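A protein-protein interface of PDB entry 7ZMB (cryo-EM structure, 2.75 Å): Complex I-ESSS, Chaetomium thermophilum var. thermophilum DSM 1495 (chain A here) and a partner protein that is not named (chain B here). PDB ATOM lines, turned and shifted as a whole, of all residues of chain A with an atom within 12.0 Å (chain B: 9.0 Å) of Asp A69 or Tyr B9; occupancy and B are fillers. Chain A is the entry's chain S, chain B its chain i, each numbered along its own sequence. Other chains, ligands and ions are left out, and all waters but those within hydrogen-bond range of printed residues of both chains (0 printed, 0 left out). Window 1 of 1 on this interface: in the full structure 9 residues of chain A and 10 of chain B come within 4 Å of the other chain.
OH of Tyr B9 sits at hydrogen-bond distance from NZ of Lys B11 (2.8 Å).
The side-chain hydroxyl (OH) of Tyr B21 is in hydrogen-bond range of the backbone NH (N) of Ile B7 (3.4 Å).
Of the 17 printed residues of chain B, 9 touch a printed residue of chain A.
Among the printed residues, Asp or Glu carboxylates within 4 Å of a Lys or Arg side-chain nitrogen of the other chain: Asp A69 with Lys B6.
Among the printed residues, merely in contact across the chains: Gln A67 with Lys B6 (3.6 Å), Tyr A68 with Tyr B21 (3.4 Å), Tyr A68 with Gln B23 (3.0 Å), Asp A69 with Ala B22 (3.5 Å), Pro A70 with Gln B23 (3.5 Å), Pro A71 with Ala B22 (3.8 Å), Pro A71 with Gln B23 (3.3 Å), Pro A71 with Pro B24 (3.4 Å), Thr A72 with Val B13 (3.6 Å), Gly A73 with His B12 (3.4 Å) and Gly A73 with Val B13 (3.7 Å).
Of chain B, only Lys B6 (3.6 Å), Tyr B9 (2.6 Å), Tyr B21 (2.7 Å), Ala B22 (3.5 Å) and Gln B23 (2.9 Å) come within 4 Å of Asp A69.
Tyr B9 touches just one residue of chain A: Asp A69 (2.6 Å).
No residue of chain A comes within 4 Å of Pro B8.
Lys B11 touches just these residues of chain A: Thr A72 (3.3 Å) and Gly A73 (3.4 Å).
Val B13 touches just these residues of chain A: Thr A72 (3.6 Å) and Gly A73 (3.7 Å).
No residue of chain A comes within 4 Å of Gly B19.
Trp B20 touches none of the printed residues of chain A.
Tyr B21 touches just these residues of chain A: Tyr A68 and Asp A69.
Pro B24 touches one residue of chain A.
Printed residues of chain B within 4 Å of Gly A73: Lys B11, His B12 and Val B13.
Of the printed residues of chain B, Thr A72 touches Lys B11 (3.3 Å) and Val B13 (3.6 Å).
The nearest residue of chain A that does not touch Tyr B9 is Thr A72 (5.1 Å).
The backbone carbonyl oxygen (O) of Tyr B21 lies within hydrogen-bond range of the backbone NH (N) of Asp A69.
O of His B12 sits at hydrogen-bond distance from N of Trp A74, at 2.6 Å.
The backbone carbonyl oxygen (O) of Asp A69 lies within hydrogen-bond range of the backbone NH (N) of Gln B23 (2.9 Å).
The backbone NH of Gly A73 sits at hydrogen-bond distance from the backbone carbonyl oxygen of Lys B11, at 3.4 Å.
The side-chain hydroxyl (OG1) of Thr A72 sits at hydrogen-bond distance from the backbone carbonyl oxygen (O) of Lys B11, 3.3 Å away.
OD1 of Asp A69 is in salt-bridge range of NZ of Lys B6 (3.8 Å).
OD2 of Asp A69 is in hydrogen-bond range of OH of Tyr B9 (2.6 Å).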
ATOM      1  N   GLN A  67      15.455   1.625  20.650  1.00  0.00           N
ATOM      2  CA  GLN A  67      16.738   0.954  20.497  1.00  0.00           C
ATOM      3  C   GLN A  67      17.511   1.502  19.305  1.00  0.00           C
ATOM      4  O   GLN A  67      17.021   2.363  18.577  1.00  0.00           O
ATOM      5  CB  GLN A  67      16.540  -0.554  20.344  1.00  0.00           C
ATOM      6  CG  GLN A  67      16.070  -1.243  21.610  1.00  0.00           C
ATOM      7  CD  GLN A  67      17.072  -1.120  22.743  1.00  0.00           C
ATOM      8  OE1 GLN A  67      18.283  -1.148  22.521  1.00  0.00           O
ATOM      9  NE2 GLN A  67      16.572  -0.983  23.965  1.00  0.00           N
ATOM     10  N   TYR A  68      18.727   0.996  19.116  1.00  0.00           N
ATOM     11  CA  TYR A  68      19.615   1.440  18.049  1.00  0.00           C
ATOM     12  C   TYR A  68      20.243   0.216  17.407  1.00  0.00           C
ATOM     13  O   TYR A  68      20.924  -0.560  18.084  1.00  0.00           O
ATOM     14  CB  TYR A  68      20.680   2.387  18.593  1.00  0.00           C
ATOM     15  CG  TYR A  68      20.163   3.781  18.835  1.00  0.00           C
ATOM     16  CD1 TYR A  68      19.462   4.457  17.852  1.00  0.00           C
ATOM     17  CD2 TYR A  68      20.321   4.396  20.065  1.00  0.00           C
ATOM     18  CE1 TYR A  68      18.974   5.727  18.072  1.00  0.00           C
ATOM     19  CE2 TYR A  68      19.837   5.665  20.297  1.00  0.00           C
ATOM     20  CZ  TYR A  68      19.161   6.327  19.298  1.00  0.00           C
ATOM     21  OH  TYR A  68      18.672   7.592  19.526  1.00  0.00           O
ATOM     22  N   ASP A  69      20.012   0.044  16.113  1.00  0.00           N
ATOM     23  CA  ASP A  69      20.436  -1.162  15.427  1.00  0.00           C
ATOM     24  C   ASP A  69      21.945  -1.162  15.202  1.00  0.00           C
ATOM     25  O   ASP A  69      22.547  -0.108  14.987  1.00  0.00           O
ATOM     26  CB  ASP A  69      19.718  -1.290  14.088  1.00  0.00           C
ATOM     27  CG  ASP A  69      18.247  -1.613  14.246  1.00  0.00           C
ATOM     28  OD1 ASP A  69      17.863  -2.125  15.318  1.00  0.00           O
ATOM     29  OD2 ASP A  69      17.474  -1.350  13.300  1.00  0.00           O
ATOM     30  N   PRO A  70      22.576  -2.329  15.251  1.00  0.00           N
ATOM     31  CA  PRO A  70      23.995  -2.417  14.912  1.00  0.00           C
ATOM     32  C   PRO A  70      24.222  -1.991  13.475  1.00  0.00           C
ATOM     33  O   PRO A  70      23.428  -2.332  12.585  1.00  0.00           O
ATOM     34  CB  PRO A  70      24.316  -3.906  15.111  1.00  0.00           C
ATOM     35  CG  PRO A  70      23.000  -4.593  14.982  1.00  0.00           C
ATOM     36  CD  PRO A  70      22.006  -3.646  15.578  1.00  0.00           C
ATOM     37  N   PRO A  71      25.295  -1.255  13.203  1.00  0.00           N
ATOM     38  CA  PRO A  71      25.513  -0.750  11.846  1.00  0.00           C
ATOM     39  C   PRO A  71      25.942  -1.870  10.918  1.00  0.00           C
ATOM     40  O   PRO A  71      26.773  -2.712  11.264  1.00  0.00           O
ATOM     41  CB  PRO A  71      26.626   0.292  12.023  1.00  0.00           C
ATOM     42  CG  PRO A  71      27.155   0.108  13.414  1.00  0.00           C
ATOM     43  CD  PRO A  71      26.461  -1.037  14.066  1.00  0.00           C
ATOM     44  N   THR A  72      25.357  -1.873   9.724  1.00  0.00           N
ATOM     45  CA  THR A  72      25.600  -2.926   8.753  1.00  0.00           C
ATOM     46  C   THR A  72      25.630  -2.316   7.362  1.00  0.00           C
ATOM     47  O   THR A  72      25.350  -1.129   7.169  1.00  0.00           O
ATOM     48  CB  THR A  72      24.534  -4.022   8.834  1.00  0.00           C
ATOM     49  OG1 THR A  72      24.904  -5.108   7.976  1.00  0.00           O
ATOM     50  CG2 THR A  72      23.188  -3.480   8.388  1.00  0.00           C
ATOM     51  N   GLY A  73      25.956  -3.146   6.392  1.00  0.00           N
ATOM     52  CA  GLY A  73      26.083  -2.743   5.007  1.00  0.00           C
ATOM     53  C   GLY A  73      27.209  -3.524   4.371  1.00  0.00           C
ATOM     54  O   GLY A  73      28.083  -4.071   5.040  1.00  0.00           O
ATOM     55  N   TRP A  74      27.185  -3.587   3.052  1.00  0.00           N
ATOM     56  CA  TRP A  74      28.173  -4.336   2.285  1.00  0.00           C
ATOM     57  C   TRP A  74      28.990  -3.326   1.493  1.00  0.00           C
ATOM     58  O   TRP A  74      28.585  -2.914   0.402  1.00  0.00           O
ATOM     59  CB  TRP A  74      27.498  -5.345   1.361  1.00  0.00           C
ATOM     60  CG  TRP A  74      26.669  -6.379   2.067  1.00  0.00           C
ATOM     61  CD1 TRP A  74      26.570  -6.575   3.414  1.00  0.00           C
ATOM     62  CD2 TRP A  74      25.829  -7.362   1.456  1.00  0.00           C
ATOM     63  NE1 TRP A  74      25.715  -7.616   3.677  1.00  0.00           N
ATOM     64  CE2 TRP A  74      25.248  -8.117   2.491  1.00  0.00           C
ATOM     65  CE3 TRP A  74      25.510  -7.677   0.133  1.00  0.00           C
ATOM     66  CZ2 TRP A  74      24.368  -9.166   2.245  1.00  0.00           C
ATOM     67  CZ3 TRP A  74      24.637  -8.717  -0.110  1.00  0.00           C
ATOM     68  CH2 TRP A  74      24.076  -9.450   0.941  1.00  0.00           C
ATOM     69  N   PRO B   5       7.358   2.599  16.178  1.00  0.00           N
ATOM     70  CA  PRO B   5       7.925   1.401  15.565  1.00  0.00           C
ATOM     71  C   PRO B   5       9.271   1.655  14.893  1.00  0.00           C
ATOM     72  O   PRO B   5       9.914   2.668  15.164  1.00  0.00           O
ATOM     73  CB  PRO B   5       6.858   1.030  14.538  1.00  0.00           C
ATOM     74  CG  PRO B   5       6.244   2.398  14.132  1.00  0.00           C
ATOM     75  CD  PRO B   5       6.739   3.437  15.140  1.00  0.00           C
ATOM     76  N   LYS B   6       9.688   0.736  14.026  1.00  0.00           N
ATOM     77  CA  LYS B   6      10.951   0.860  13.311  1.00  0.00           C
ATOM     78  C   LYS B   6      10.721   0.537  11.844  1.00  0.00           C
ATOM     79  O   LYS B   6      10.156  -0.510  11.517  1.00  0.00           O
ATOM     80  CB  LYS B   6      12.015  -0.072  13.902  1.00  0.00           C
ATOM     81  CG  LYS B   6      13.438   0.408  13.696  1.00  0.00           C
ATOM     82  CD  LYS B   6      14.387  -0.240  14.687  1.00  0.00           C
ATOM     83  CE  LYS B   6      14.001   0.099  16.118  1.00  0.00           C
ATOM     84  NZ  LYS B   6      14.978  -0.439  17.103  1.00  0.00           N
ATOM     85  N   ILE B   7      11.157   1.433  10.970  1.00  0.00           N
ATOM     86  CA  ILE B   7      10.951   1.240   9.530  1.00  0.00           C
ATOM     87  C   ILE B   7      11.868   0.127   9.034  1.00  0.00           C
ATOM     88  O   ILE B   7      13.074   0.147   9.333  1.00  0.00           O
ATOM     89  CB  ILE B   7      11.218   2.542   8.778  1.00  0.00           C
ATOM     90  CG1 ILE B   7      10.508   3.709   9.463  1.00  0.00           C
ATOM     91  CG2 ILE B   7      10.774   2.418   7.331  1.00  0.00           C
ATOM     92  CD1 ILE B   7       9.004   3.680   9.313  1.00  0.00           C
ATOM     93  N   PRO B   8      11.362  -0.856   8.296  1.00  0.00           N
ATOM     94  CA  PRO B   8      12.255  -1.841   7.682  1.00  0.00           C
ATOM     95  C   PRO B   8      13.128  -1.190   6.623  1.00  0.00           C
ATOM     96  O   PRO B   8      12.744  -0.206   5.987  1.00  0.00           O
ATOM     97  CB  PRO B   8      11.293  -2.859   7.063  1.00  0.00           C
ATOM     98  CG  PRO B   8      10.046  -2.088   6.827  1.00  0.00           C
ATOM     99  CD  PRO B   8       9.953  -1.100   7.954  1.00  0.00           C
ATOM    100  N   TYR B   9      14.320  -1.747   6.439  1.00  0.00           N
ATOM    101  CA  TYR B   9      15.290  -1.171   5.521  1.00  0.00           C
ATOM    102  C   TYR B   9      16.276  -2.253   5.117  1.00  0.00           C
ATOM    103  O   TYR B   9      16.447  -3.239   5.844  1.00  0.00           O
ATOM    104  CB  TYR B   9      16.016   0.015   6.164  1.00  0.00           C
ATOM    105  CG  TYR B   9      16.715  -0.332   7.446  1.00  0.00           C
ATOM    106  CD1 TYR B   9      18.010  -0.819   7.440  1.00  0.00           C
ATOM    107  CD2 TYR B   9      16.083  -0.166   8.665  1.00  0.00           C
ATOM    108  CE1 TYR B   9      18.648  -1.131   8.605  1.00  0.00           C
ATOM    109  CE2 TYR B   9      16.719  -0.483   9.836  1.00  0.00           C
ATOM    110  CZ  TYR B   9      18.003  -0.960   9.799  1.00  0.00           C
ATOM    111  OH  TYR B   9      18.643  -1.276  10.970  1.00  0.00           O
ATOM    112  N   PRO B  10      16.944  -2.098   3.972  1.00  0.00           N
ATOM    113  CA  PRO B  10      17.913  -3.110   3.543  1.00  0.00           C
ATOM    114  C   PRO B  10      19.104  -3.183   4.477  1.00  0.00           C
ATOM    115  O   PRO B  10      19.493  -2.200   5.107  1.00  0.00           O
ATOM    116  CB  PRO B  10      18.345  -2.630   2.153  1.00  0.00           C
ATOM    117  CG  PRO B  10      17.408  -1.559   1.781  1.00  0.00           C
ATOM    118  CD  PRO B  10      16.899  -0.963   3.041  1.00  0.00           C
ATOM    119  N   LYS B  11      19.696  -4.369   4.552  1.00  0.00           N
ATOM    120  CA  LYS B  11      20.862  -4.586   5.393  1.00  0.00           C
ATOM    121  C   LYS B  11      22.159  -4.599   4.602  1.00  0.00           C
ATOM    122  O   LYS B  11      23.231  -4.746   5.195  1.00  0.00           O
ATOM    123  CB  LYS B  11      20.711  -5.895   6.172  1.00  0.00           C
ATOM    124  CG  LYS B  11      19.515  -5.902   7.109  1.00  0.00           C
ATOM    125  CD  LYS B  11      19.693  -4.912   8.244  1.00  0.00           C
ATOM    126  CE  LYS B  11      18.530  -4.981   9.218  1.00  0.00           C
ATOM    127  NZ  LYS B  11      18.661  -3.988  10.318  1.00  0.00           N
ATOM    128  N   HIS B  12      22.093  -4.432   3.289  1.00  0.00           N
ATOM    129  CA  HIS B  12      23.282  -4.448   2.457  1.00  0.00           C
ATOM    130  C   HIS B  12      23.846  -3.063   2.194  1.00  0.00           C
ATOM    131  O   HIS B  12      24.994  -2.953   1.752  1.00  0.00           O
ATOM    132  CB  HIS B  12      22.978  -5.126   1.127  1.00  0.00           C
ATOM    133  CG  HIS B  12      21.699  -4.676   0.494  1.00  0.00           C
ATOM    134  ND1 HIS B  12      21.661  -3.757  -0.532  1.00  0.00           N
ATOM    135  CD2 HIS B  12      20.417  -5.043   0.717  1.00  0.00           C
ATOM    136  CE1 HIS B  12      20.410  -3.567  -0.906  1.00  0.00           C
ATOM    137  NE2 HIS B  12      19.635  -4.338  -0.167  1.00  0.00           N
ATOM    138  N   VAL B  13      23.088  -2.011   2.487  1.00  0.00           N
ATOM    139  CA  VAL B  13      23.409  -0.666   2.031  1.00  0.00           C
ATOM    140  C   VAL B  13      24.430  -0.068   2.996  1.00  0.00           C
ATOM    141  O   VAL B  13      24.093   0.365   4.095  1.00  0.00           O
ATOM    142  CB  VAL B  13      22.151   0.192   1.915  1.00  0.00           C
ATOM    143  CG1 VAL B  13      22.507   1.615   1.611  1.00  0.00           C
ATOM    144  CG2 VAL B  13      21.243  -0.367   0.840  1.00  0.00           C
ATOM    145  N   GLY B  18      26.381   5.941   8.406  1.00  0.00           N
ATOM    146  CA  GLY B  18      25.954   4.924   9.338  1.00  0.00           C
ATOM    147  C   GLY B  18      24.837   4.020   8.880  1.00  0.00           C
ATOM    148  O   GLY B  18      24.860   2.816   9.156  1.00  0.00           O
ATOM    149  N   GLY B  19      23.861   4.565   8.175  1.00  0.00           N
ATOM    150  CA  GLY B  19      22.750   3.739   7.757  1.00  0.00           C
ATOM    151  C   GLY B  19      21.467   4.168   8.432  1.00  0.00           C
ATOM    152  O   GLY B  19      21.262   5.363   8.653  1.00  0.00           O
ATOM    153  N   TRP B  20      20.597   3.220   8.778  1.00  0.00           N
ATOM    154  CA  TRP B  20      19.281   3.617   9.260  1.00  0.00           C
ATOM    155  C   TRP B  20      19.271   3.886  10.758  1.00  0.00           C
ATOM    156  O   TRP B  20      19.061   5.022  11.175  1.00  0.00           O
ATOM    157  CB  TRP B  20      18.241   2.564   8.884  1.00  0.00           C
ATOM    158  CG  TRP B  20      17.678   2.836   7.559  1.00  0.00           C
ATOM    159  CD1 TRP B  20      16.496   3.438   7.281  1.00  0.00           C
ATOM    160  CD2 TRP B  20      18.297   2.558   6.307  1.00  0.00           C
ATOM    161  NE1 TRP B  20      16.325   3.536   5.925  1.00  0.00           N
ATOM    162  CE2 TRP B  20      17.421   3.003   5.303  1.00  0.00           C
ATOM    163  CE3 TRP B  20      19.504   1.962   5.937  1.00  0.00           C
ATOM    164  CZ2 TRP B  20      17.707   2.868   3.960  1.00  0.00           C
ATOM    165  CZ3 TRP B  20      19.788   1.831   4.606  1.00  0.00           C
ATOM    166  CH2 TRP B  20      18.894   2.277   3.630  1.00  0.00           C
ATOM    167  N   TYR B  21      19.539   2.882  11.581  1.00  0.00           N
ATOM    168  CA  TYR B  21      19.528   3.155  13.013  1.00  0.00           C
ATOM    169  C   TYR B  21      20.879   2.805  13.606  1.00  0.00           C
ATOM    170  O   TYR B  21      20.964   2.130  14.636  1.00  0.00           O
ATOM    171  CB  TYR B  21      18.401   2.390  13.701  1.00  0.00           C
ATOM    172  CG  TYR B  21      17.032   2.787  13.206  1.00  0.00           C
ATOM    173  CD1 TYR B  21      16.473   2.180  12.097  1.00  0.00           C
ATOM    174  CD2 TYR B  21      16.301   3.770  13.849  1.00  0.00           C
ATOM    175  CE1 TYR B  21      15.234   2.541  11.640  1.00  0.00           C
ATOM    176  CE2 TYR B  21      15.058   4.138  13.402  1.00  0.00           C
ATOM    177  CZ  TYR B  21      14.527   3.520  12.299  1.00  0.00           C
ATOM    178  OH  TYR B  21      13.282   3.886  11.849  1.00  0.00           O
ATOM    179  N   ALA B  22      21.934   3.276  12.957  1.00  0.00           N
ATOM    180  CA  ALA B  22      23.271   2.770  13.209  1.00  0.00           C
ATOM    181  C   ALA B  22      23.787   3.168  14.584  1.00  0.00           C
ATOM    182  O   ALA B  22      23.747   4.340  14.964  1.00  0.00           O
ATOM    183  CB  ALA B  22      24.225   3.276  12.139  1.00  0.00           C
ATOM    184  N   GLN B  23      24.263   2.178  15.325  1.00  0.00           N
ATOM    185  CA  GLN B  23      25.148   2.413  16.452  1.00  0.00           C
ATOM    186  C   GLN B  23      25.957   1.153  16.714  1.00  0.00           C
ATOM    187  O   GLN B  23      25.383   0.091  16.979  1.00  0.00           O
ATOM    188  CB  GLN B  23      24.380   2.833  17.705  1.00  0.00           C
ATOM    189  CG  GLN B  23      25.302   3.290  18.819  1.00  0.00           C
ATOM    190  CD  GLN B  23      24.649   4.279  19.754  1.00  0.00           C
ATOM    191  OE1 GLN B  23      25.318   5.102  20.379  1.00  0.00           O
ATOM    192  NE2 GLN B  23      23.331   4.204  19.857  1.00  0.00           N
ATOM    193  N   PRO B  24      27.308   1.230  16.649  1.00  0.00           N
ATOM    194  CA  PRO B  24      28.133   0.076  16.975  1.00  0.00           C
ATOM    195  C   PRO B  24      28.180  -0.221  18.479  1.00  0.00           C
ATOM    196  O   PRO B  24      27.856   0.657  19.258  1.00  0.00           O
ATOM    197  CB  PRO B  24      29.508   0.470  16.441  1.00  0.00           C
ATOM    198  CG  PRO B  24      29.559   1.953  16.616  1.00  0.00           C
ATOM    199  CD  PRO B  24      28.162   2.373  16.234  1.00  0.00           C
ATOM    200  N   ALA B  25      28.567  -1.443  18.844  1.00  0.00           N
ATOM    201  CA  ALA B  25      28.723  -1.807  20.273  1.00  0.00           C
ATOM    202  C   ALA B  25      29.862  -0.984  20.871  1.00  0.00           C
ATOM    203  O   ALA B  25      29.845  -0.771  22.098  1.00  0.00           O
ATOM    204  CB  ALA B  25      29.011  -3.278  20.397  1.00  0.00           C
